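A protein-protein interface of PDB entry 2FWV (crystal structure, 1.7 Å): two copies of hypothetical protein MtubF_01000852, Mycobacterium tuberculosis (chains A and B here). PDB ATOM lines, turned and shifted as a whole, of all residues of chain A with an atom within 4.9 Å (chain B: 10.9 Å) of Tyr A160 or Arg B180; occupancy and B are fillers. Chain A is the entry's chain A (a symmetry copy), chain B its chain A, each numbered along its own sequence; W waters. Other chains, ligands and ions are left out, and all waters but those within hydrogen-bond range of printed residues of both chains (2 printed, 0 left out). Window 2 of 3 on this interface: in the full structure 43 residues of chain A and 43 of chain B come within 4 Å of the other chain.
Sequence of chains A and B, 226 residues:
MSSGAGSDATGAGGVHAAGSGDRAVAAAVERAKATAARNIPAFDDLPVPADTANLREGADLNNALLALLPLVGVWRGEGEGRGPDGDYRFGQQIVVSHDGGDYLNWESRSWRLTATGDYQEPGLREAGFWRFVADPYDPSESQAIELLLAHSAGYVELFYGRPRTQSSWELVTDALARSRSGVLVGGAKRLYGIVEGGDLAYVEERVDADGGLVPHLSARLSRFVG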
ATOM      1  N   VAL A 133      14.390  11.023 -15.327  1.00  0.00           N
ATOM      2  CA  VAL A 133      15.724  11.655 -15.378  1.00  0.00           C
ATOM      3  C   VAL A 133      15.703  13.020 -16.050  1.00  0.00           C
ATOM      4  O   VAL A 133      14.680  13.692 -16.061  1.00  0.00           O
ATOM      5  CB  VAL A 133      16.778  10.756 -16.123  1.00  0.00           C
ATOM      6  CG1 VAL A 133      16.178  10.068 -17.376  1.00  0.00           C
ATOM      7  CG2 VAL A 133      18.072  11.546 -16.437  1.00  0.00           C
ATOM      8  N   ALA A 144      11.547  14.732 -14.097  1.00  0.00           N
ATOM      9  CA  ALA A 144      10.907  14.576 -15.446  1.00  0.00           C
ATOM     10  C   ALA A 144      10.848  13.141 -15.986  1.00  0.00           C
ATOM     11  O   ALA A 144      11.817  12.361 -15.907  1.00  0.00           O
ATOM     12  CB  ALA A 144      11.505  15.492 -16.497  1.00  0.00           C
ATOM     13  N   ILE A 145       9.705  12.831 -16.584  1.00  0.00           N
ATOM     14  CA  ILE A 145       9.389  11.469 -17.090  1.00  0.00           C
ATOM     15  C   ILE A 145       9.453  11.551 -18.627  1.00  0.00           C
ATOM     16  O   ILE A 145       9.066  12.577 -19.205  1.00  0.00           O
ATOM     17  CB  ILE A 145       7.937  11.030 -16.717  1.00  0.00           C
ATOM     18  CG1 ILE A 145       7.652  11.059 -15.206  1.00  0.00           C
ATOM     19  CG2 ILE A 145       7.652   9.587 -17.234  1.00  0.00           C
ATOM     20  CD1 ILE A 145       6.117  10.841 -14.902  1.00  0.00           C
ATOM     21  N   GLU A 146       9.930  10.488 -19.269  1.00  0.00           N
ATOM     22  CA  GLU A 146       9.943  10.402 -20.750  1.00  0.00           C
ATOM     23  C   GLU A 146       9.243   9.072 -21.086  1.00  0.00           C
ATOM     24  O   GLU A 146       9.478   8.080 -20.407  1.00  0.00           O
ATOM     25  CB  GLU A 146      11.412  10.332 -21.219  1.00  0.00           C
ATOM     26  CG  GLU A 146      12.337  11.403 -20.556  1.00  0.00           C
ATOM     27  CD  GLU A 146      13.829  11.184 -20.781  1.00  0.00           C
ATOM     28  OE1 GLU A 146      14.243  10.115 -21.287  1.00  0.00           O
ATOM     29  OE2 GLU A 146      14.603  12.102 -20.413  1.00  0.00           O
ATOM     30  N   LEU A 158       7.070  10.620 -28.961  1.00  0.00           N
ATOM     31  CA  LEU A 158       7.828  10.960 -27.750  1.00  0.00           C
ATOM     32  C   LEU A 158       6.864  11.731 -26.831  1.00  0.00           C
ATOM     33  O   LEU A 158       6.221  12.680 -27.251  1.00  0.00           O
ATOM     34  CB  LEU A 158       9.032  11.819 -28.142  1.00  0.00           C
ATOM     35  CG  LEU A 158       9.826  12.375 -26.957  1.00  0.00           C
ATOM     36  CD1 LEU A 158      10.347  11.218 -26.098  1.00  0.00           C
ATOM     37  CD2 LEU A 158      10.989  13.148 -27.613  1.00  0.00           C
ATOM     38  N   PHE A 159       6.791  11.299 -25.572  1.00  0.00           N
ATOM     39  CA  PHE A 159       5.982  11.977 -24.514  1.00  0.00           C
ATOM     40  C   PHE A 159       6.977  12.480 -23.471  1.00  0.00           C
ATOM     41  O   PHE A 159       7.987  11.815 -23.172  1.00  0.00           O
ATOM     42  CB  PHE A 159       5.065  10.994 -23.764  1.00  0.00           C
ATOM     43  CG  PHE A 159       3.798  10.602 -24.500  1.00  0.00           C
ATOM     44  CD1 PHE A 159       2.642  11.367 -24.393  1.00  0.00           C
ATOM     45  CD2 PHE A 159       3.754   9.441 -25.255  1.00  0.00           C
ATOM     46  CE1 PHE A 159       1.453  11.001 -25.019  1.00  0.00           C
ATOM     47  CE2 PHE A 159       2.579   9.082 -25.879  1.00  0.00           C
ATOM     48  CZ  PHE A 159       1.438   9.854 -25.771  1.00  0.00           C
ATOM     49  N   TYR A 160       6.671  13.633 -22.903  1.00  0.00           N
ATOM     50  CA  TYR A 160       7.442  14.154 -21.784  1.00  0.00           C
ATOM     51  C   TYR A 160       6.466  14.558 -20.686  1.00  0.00           C
ATOM     52  O   TYR A 160       5.338  14.972 -20.970  1.00  0.00           O
ATOM     53  CB  TYR A 160       8.160  15.372 -22.323  1.00  0.00           C
ATOM     54  CG  TYR A 160       8.798  16.211 -21.298  1.00  0.00           C
ATOM     55  CD1 TYR A 160       8.085  17.244 -20.670  1.00  0.00           C
ATOM     56  CD2 TYR A 160      10.121  15.993 -20.945  1.00  0.00           C
ATOM     57  CE1 TYR A 160       8.691  18.044 -19.686  1.00  0.00           C
ATOM     58  CE2 TYR A 160      10.736  16.781 -19.975  1.00  0.00           C
ATOM     59  CZ  TYR A 160      10.018  17.793 -19.345  1.00  0.00           C
ATOM     60  OH  TYR A 160      10.651  18.566 -18.383  1.00  0.00           O
ATOM     61  N   GLY A 161       6.875  14.420 -19.426  1.00  0.00           N
ATOM     62  CA  GLY A 161       5.952  14.830 -18.378  1.00  0.00           C
ATOM     63  C   GLY A 161       6.556  14.791 -17.010  1.00  0.00           C
ATOM     64  O   GLY A 161       7.785  14.905 -16.848  1.00  0.00           O
ATOM     65  N   ARG A 162       5.668  14.604 -16.038  1.00  0.00           N
ATOM     66  CA  ARG A 162       6.081  14.680 -14.637  1.00  0.00           C
ATOM     67  C   ARG A 162       5.181  13.857 -13.730  1.00  0.00           C
ATOM     68  O   ARG A 162       3.994  13.615 -14.031  1.00  0.00           O
ATOM     69  CB  ARG A 162       6.059  16.133 -14.205  1.00  0.00           C
ATOM     70  CG  ARG A 162       4.690  16.759 -14.309  1.00  0.00           C
ATOM     71  CD  ARG A 162       4.677  18.160 -13.668  1.00  0.00           C
ATOM     72  NE  ARG A 162       5.910  18.916 -13.929  1.00  0.00           N
ATOM     73  CZ  ARG A 162       6.296  20.015 -13.264  1.00  0.00           C
ATOM     74  NH1 ARG A 162       5.551  20.514 -12.271  1.00  0.00           N
ATOM     75  NH2 ARG A 162       7.436  20.620 -13.593  1.00  0.00           N
ATOM     76  N   GLU A 170       1.713  12.346 -15.410  1.00  0.00           N
ATOM     77  CA  GLU A 170       1.102  13.066 -16.527  1.00  0.00           C
ATOM     78  C   GLU A 170       2.146  13.208 -17.645  1.00  0.00           C
ATOM     79  O   GLU A 170       3.290  13.536 -17.357  1.00  0.00           O
ATOM     80  CB  GLU A 170       0.625  14.445 -16.052  1.00  0.00           C
ATOM     81  CG  GLU A 170       0.063  15.332 -17.139  1.00  0.00           C
ATOM     82  CD  GLU A 170      -0.205  16.770 -16.661  1.00  0.00           C
ATOM     83  OE1 GLU A 170      -0.781  16.946 -15.564  1.00  0.00           O
ATOM     84  OE2 GLU A 170       0.165  17.706 -17.405  1.00  0.00           O
ATOM     85  N   LEU A 171       1.758  12.957 -18.905  1.00  0.00           N
ATOM     86  CA  LEU A 171       2.673  12.993 -20.023  1.00  0.00           C
ATOM     87  C   LEU A 171       1.980  13.683 -21.173  1.00  0.00           C
ATOM     88  O   LEU A 171       0.786  13.527 -21.329  1.00  0.00           O
ATOM     89  CB  LEU A 171       2.953  11.532 -20.502  1.00  0.00           C
ATOM     90  CG  LEU A 171       3.800  10.578 -19.642  1.00  0.00           C
ATOM     91  CD1 LEU A 171       3.437   9.124 -19.989  1.00  0.00           C
ATOM     92  CD2 LEU A 171       5.282  10.802 -19.901  1.00  0.00           C
ATOM     93  N   VAL A 172       2.731  14.437 -21.976  1.00  0.00           N
ATOM     94  CA  VAL A 172       2.179  15.107 -23.161  1.00  0.00           C
ATOM     95  C   VAL A 172       3.093  14.851 -24.363  1.00  0.00           C
ATOM     96  O   VAL A 172       4.319  14.797 -24.218  1.00  0.00           O
ATOM     97  CB  VAL A 172       1.977  16.662 -22.916  1.00  0.00           C
ATOM     98  CG1 VAL A 172       1.594  17.353 -24.187  1.00  0.00           C
ATOM     99  CG2 VAL A 172       0.952  16.873 -21.805  1.00  0.00           C
ATOM    100  N   ASP A 174       5.465  15.377 -27.405  1.00  0.00           N
ATOM    101  CA  ASP A 174       6.383  16.371 -27.908  1.00  0.00           C
ATOM    102  C   ASP A 174       6.851  16.090 -29.333  1.00  0.00           C
ATOM    103  O   ASP A 174       7.364  16.988 -29.984  1.00  0.00           O
ATOM    104  CB  ASP A 174       7.630  16.492 -26.998  1.00  0.00           C
ATOM    105  CG  ASP A 174       7.426  17.432 -25.842  1.00  0.00           C
ATOM    106  OD1 ASP A 174       6.348  18.050 -25.741  1.00  0.00           O
ATOM    107  OD2 ASP A 174       8.387  17.571 -25.040  1.00  0.00           O
ATOM    108  N   HIS B 151      14.002   3.415 -28.459  1.00  0.00           N
ATOM    109  CA  HIS B 151      15.289   2.951 -27.986  1.00  0.00           C
ATOM    110  C   HIS B 151      15.411   3.227 -26.491  1.00  0.00           C
ATOM    111  O   HIS B 151      15.112   4.343 -26.076  1.00  0.00           O
ATOM    112  CB  HIS B 151      16.420   3.721 -28.664  1.00  0.00           C
ATOM    113  CG  HIS B 151      16.557   3.449 -30.141  1.00  0.00           C
ATOM    114  ND1 HIS B 151      17.384   2.462 -30.638  1.00  0.00           N
ATOM    115  CD2 HIS B 151      16.020   4.078 -31.210  1.00  0.00           C
ATOM    116  CE1 HIS B 151      17.336   2.484 -31.968  1.00  0.00           C
ATOM    117  NE2 HIS B 151      16.524   3.462 -32.336  1.00  0.00           N
ATOM    118  N   SER B 152      15.896   2.242 -25.742  1.00  0.00           N
ATOM    119  CA  SER B 152      16.011   2.393 -24.251  1.00  0.00           C
ATOM    120  C   SER B 152      16.923   3.548 -23.877  1.00  0.00           C
ATOM    121  O   SER B 152      16.773   4.131 -22.763  1.00  0.00           O
ATOM    122  CB  SER B 152      16.498   1.064 -23.636  1.00  0.00           C
ATOM    123  OG  SER B 152      17.801   0.729 -24.106  1.00  0.00           O
ATOM    124  N   ALA B 153      17.876   3.865 -24.764  1.00  0.00           N
ATOM    125  CA  ALA B 153      18.835   4.984 -24.547  1.00  0.00           C
ATOM    126  C   ALA B 153      18.180   6.357 -24.606  1.00  0.00           C
ATOM    127  O   ALA B 153      18.867   7.405 -24.384  1.00  0.00           O
ATOM    128  CB  ALA B 153      20.000   4.903 -25.536  1.00  0.00           C
ATOM    129  N   GLY B 154      16.903   6.408 -24.998  1.00  0.00           N
ATOM    130  CA  GLY B 154      16.150   7.654 -24.925  1.00  0.00           C
ATOM    131  C   GLY B 154      15.897   8.389 -26.240  1.00  0.00           C
ATOM    132  O   GLY B 154      15.833   9.648 -26.277  1.00  0.00           O
ATOM    133  N   TYR B 155      15.614   7.622 -27.299  1.00  0.00           N
ATOM    134  CA  TYR B 155      15.131   8.312 -28.509  1.00  0.00           C
ATOM    135  C   TYR B 155      14.211   7.386 -29.299  1.00  0.00           C
ATOM    136  O   TYR B 155      14.197   6.180 -29.030  1.00  0.00           O
ATOM    137  CB  TYR B 155      16.301   8.832 -29.346  1.00  0.00           C
ATOM    138  CG  TYR B 155      17.247   7.785 -29.933  1.00  0.00           C
ATOM    139  CD1 TYR B 155      18.240   7.177 -29.142  1.00  0.00           C
ATOM    140  CD2 TYR B 155      17.181   7.427 -31.296  1.00  0.00           C
ATOM    141  CE1 TYR B 155      19.123   6.219 -29.674  1.00  0.00           C
ATOM    142  CE2 TYR B 155      18.090   6.485 -31.850  1.00  0.00           C
ATOM    143  CZ  TYR B 155      19.053   5.885 -31.017  1.00  0.00           C
ATOM    144  OH  TYR B 155      19.946   4.964 -31.490  1.00  0.00           O
ATOM    145  N   VAL B 156      13.436   7.986 -30.201  1.00  0.00           N
ATOM    146  CA  VAL B 156      12.634   7.193 -31.174  1.00  0.00           C
ATOM    147  C   VAL B 156      13.229   7.419 -32.574  1.00  0.00           C
ATOM    148  O   VAL B 156      13.895   8.418 -32.836  1.00  0.00           O
ATOM    149  CB  VAL B 156      11.138   7.547 -31.154  1.00  0.00           C
ATOM    150  CG1 VAL B 156      10.497   7.156 -29.773  1.00  0.00           C
ATOM    151  CG2 VAL B 156      10.917   9.052 -31.435  1.00  0.00           C
ATOM    152  N   ALA B 177      14.120  11.468 -32.687  1.00  0.00           N
ATOM    153  CA  ALA B 177      13.740  12.485 -31.703  1.00  0.00           C
ATOM    154  C   ALA B 177      14.133  11.982 -30.362  1.00  0.00           C
ATOM    155  O   ALA B 177      13.826  10.834 -30.027  1.00  0.00           O
ATOM    156  CB  ALA B 177      12.251  12.754 -31.720  1.00  0.00           C
ATOM    157  N   ARG B 178      14.762  12.848 -29.575  1.00  0.00           N
ATOM    158  CA  ARG B 178      15.164  12.367 -28.252  1.00  0.00           C
ATOM    159  C   ARG B 178      14.502  13.106 -27.177  1.00  0.00           C
ATOM    160  O   ARG B 178      14.023  14.263 -27.324  1.00  0.00           O
ATOM    161  CB  ARG B 178      16.669  12.391 -28.011  1.00  0.00           C
ATOM    162  CG  ARG B 178      17.226  13.810 -27.935  1.00  0.00           C
ATOM    163  CD  ARG B 178      18.619  13.749 -27.357  1.00  0.00           C
ATOM    164  NE  ARG B 178      19.227  15.065 -27.482  1.00  0.00           N
ATOM    165  CZ  ARG B 178      20.456  15.355 -27.099  1.00  0.00           C
ATOM    166  NH1 ARG B 178      21.216  14.452 -26.498  1.00  0.00           N
ATOM    167  NH2 ARG B 178      20.905  16.573 -27.283  1.00  0.00           N
ATOM    168  N   SER B 179      14.492  12.382 -26.066  1.00  0.00           N
ATOM    169  CA  SER B 179      14.114  12.921 -24.805  1.00  0.00           C
ATOM    170  C   SER B 179      15.276  13.767 -24.274  1.00  0.00           C
ATOM    171  O   SER B 179      16.421  13.653 -24.765  1.00  0.00           O
ATOM    172  CB  SER B 179      13.935  11.732 -23.885  1.00  0.00           C
ATOM    173  OG  SER B 179      15.200  11.076 -23.851  1.00  0.00           O
ATOM    174  N   ARG B 180      15.004  14.600 -23.269  1.00  0.00           N
ATOM    175  CA  ARG B 180      16.056  15.481 -22.762  1.00  0.00           C
ATOM    176  C   ARG B 180      17.301  14.737 -22.291  1.00  0.00           C
ATOM    177  O   ARG B 180      18.425  15.223 -22.474  1.00  0.00           O
ATOM    178  CB  ARG B 180      15.552  16.426 -21.670  1.00  0.00           C
ATOM    179  CG  ARG B 180      14.626  15.803 -20.660  1.00  0.00           C
ATOM    180  CD  ARG B 180      13.769  16.892 -20.002  1.00  0.00           C
ATOM    181  NE  ARG B 180      14.248  17.268 -18.674  1.00  0.00           N
ATOM    182  CZ  ARG B 180      14.008  18.438 -18.083  1.00  0.00           C
ATOM    183  NH1 ARG B 180      13.310  19.390 -18.709  1.00  0.00           N
ATOM    184  NH2 ARG B 180      14.489  18.664 -16.863  1.00  0.00           N
ATOM    185  N   SER B 181      17.109  13.577 -21.681  1.00  0.00           N
ATOM    186  CA  SER B 181      18.256  12.840 -21.164  1.00  0.00           C
ATOM    187  C   SER B 181      18.794  11.840 -22.173  1.00  0.00           C
ATOM    188  O   SER B 181      19.766  11.120 -21.892  1.00  0.00           O
ATOM    189  CB  SER B 181      17.879  12.105 -19.889  1.00  0.00           C
ATOM    190  OG  SER B 181      17.021  11.041 -20.204  1.00  0.00           O
ATOM    191  N   GLY B 182      18.185  11.812 -23.354  1.00  0.00           N
ATOM    192  CA  GLY B 182      18.537  10.786 -24.317  1.00  0.00           C
ATOM    193  C   GLY B 182      19.885  11.036 -24.957  1.00  0.00           C
ATOM    194  O   GLY B 182      20.401  12.160 -24.942  1.00  0.00           O
ATOM    195  N   VAL B 183      20.471   9.971 -25.515  1.00  0.00           N
ATOM    196  CA  VAL B 183      21.737  10.075 -26.260  1.00  0.00           C
ATOM    197  C   VAL B 183      21.598  10.960 -27.532  1.00  0.00           C
ATOM    198  O   VAL B 183      20.510  11.062 -28.109  1.00  0.00           O
ATOM    199  CB  VAL B 183      22.318   8.647 -26.629  1.00  0.00           C
ATOM    200  CG1 VAL B 183      21.382   7.888 -27.564  1.00  0.00           C
ATOM    201  CG2 VAL B 183      23.741   8.744 -27.211  1.00  0.00           C
ATOM    202  N   LEU B 184      22.704  11.581 -27.946  1.00  0.00           N
ATOM    203  CA  LEU B 184      22.784  12.289 -29.218  1.00  0.00           C
ATOM    204  C   LEU B 184      23.273  11.331 -30.298  1.00  0.00           C
ATOM    205  O   LEU B 184      24.387  10.776 -30.190  1.00  0.00           O
ATOM    206  CB  LEU B 184      23.736  13.491 -29.123  1.00  0.00           C
ATOM    207  CG  LEU B 184      23.797  14.577 -30.219  1.00  0.00           C
ATOM    208  CD1 LEU B 184      22.451  15.294 -30.487  1.00  0.00           C
ATOM    209  CD2 LEU B 184      24.863  15.609 -29.845  1.00  0.00           C
ATOM    210  N   VAL B 185      22.477  11.172 -31.361  1.00  0.00           N
ATOM    211  CA  VAL B 185      22.873  10.265 -32.440  1.00  0.00           C
ATOM    212  C   VAL B 185      22.687  10.811 -33.847  1.00  0.00           C
ATOM    213  O   VAL B 185      22.183  11.917 -34.056  1.00  0.00           O
ATOM    214  CB  VAL B 185      22.167   8.876 -32.353  1.00  0.00           C
ATOM    215  CG1 VAL B 185      22.562   8.154 -31.080  1.00  0.00           C
ATOM    216  CG2 VAL B 185      20.655   9.038 -32.466  1.00  0.00           C
HETATM  217  O   HOH W   1      14.099  13.790 -18.586  1.00  0.00           O
HETATM  218  O   HOH W   2      10.875  21.020 -19.104  1.00  0.00           O
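Of the 13 printed residues of chain A, 5 touch a printed residue of chain B.
Printed residues of chain A that touch a printed residue of chain B: Val A133, Ala A144, Glu A146, Leu A158 and Tyr A160.
Along chain A the printed residues that touch a printed residue of chain B span positions 133 to 160.
Among the printed residues, 8 pairs touch across the chains.
Among the printed residues, no Asp or Glu carboxylate lies within 4 Å of a Lys or Arg side-chain nitrogen of the other chain.
Val A133 touches Ser B181 (CG1 to OG, 3.1 Å).
Ala A144 touches Arg B180 (CB to NE, 3.9 Å).
Glu A146 touches Arg B180.
Arg B178 touches Leu A158.
Ser B179 touches Leu A158.
No position is printed for both chains.
Of the 8 pairs that touch across the chains among the printed residues, none has its exchanged pair printed and touching as well.
Arg B180 touches just these residues of chain A: Ala A144, Glu A146 and Tyr A160.
Glu A146 touches three residues of chain B.
Leu A158 touches two residues of chain B.
No residue of chain B comes within 4 Å of Gly A161.
Of the printed residues of chain A, Arg B178 touches Leu A158.
Printed residues of chain A within 4 Å of Ser B179: Glu A146 and Leu A158.
Printed residues of chain B within 4 Å of Val A133: Ser B181 (3.1 Å).
Of the printed residues of chain A, Ser B181 touches Val A133 (3.1 Å) and Glu A146 (2.6 Å).
Ala B177 touches none of the printed residues of chain A.
Water W1 lies within hydrogen-bond range of OE2 of Glu A146, O of Val A133 and NE of Arg B180.
Water W2 lies within hydrogen-bond range of the side-chain hydroxyl (OH) of Tyr A160 (2.6 Å) and the guanidinium group (NH1) of Arg B180 (3.0 Å).
O of Gly B154 lies within hydrogen-bond range of OG of Ser B179, 2.9 Å away.
O of Gly B182 sits at hydrogen-bond distance from NH1 of Arg B178 (2.9 Å).
The side-chain hydroxyl (OG) of Ser B179 lies within hydrogen-bond range of the backbone NH (N) of Gly B182.
The backbone carbonyl oxygen of Ala A144 sits at hydrogen-bond distance from the backbone NH of Val A133 (3.0 Å).
The backbone NH (N) of Asp A174 lies within hydrogen-bond range of the backbone carbonyl oxygen (O) of Leu A158.
The backbone NH (N) of Val A172 sits at hydrogen-bond distance from the backbone carbonyl oxygen (O) of Tyr A160 (2.8 Å).
The side-chain hydroxyl of Ser B179 lies within hydrogen-bond range of the side-chain carboxylate of Glu A146 (2.9 Å).
OH of Tyr A160 lies within hydrogen-bond range of NH1 of Arg B180 (2.8 Å).
The side-chain hydroxyl (OG) of Ser B181 sits at hydrogen-bond distance from the side-chain carboxylate (OE2) of Glu A146, 2.6 Å away.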
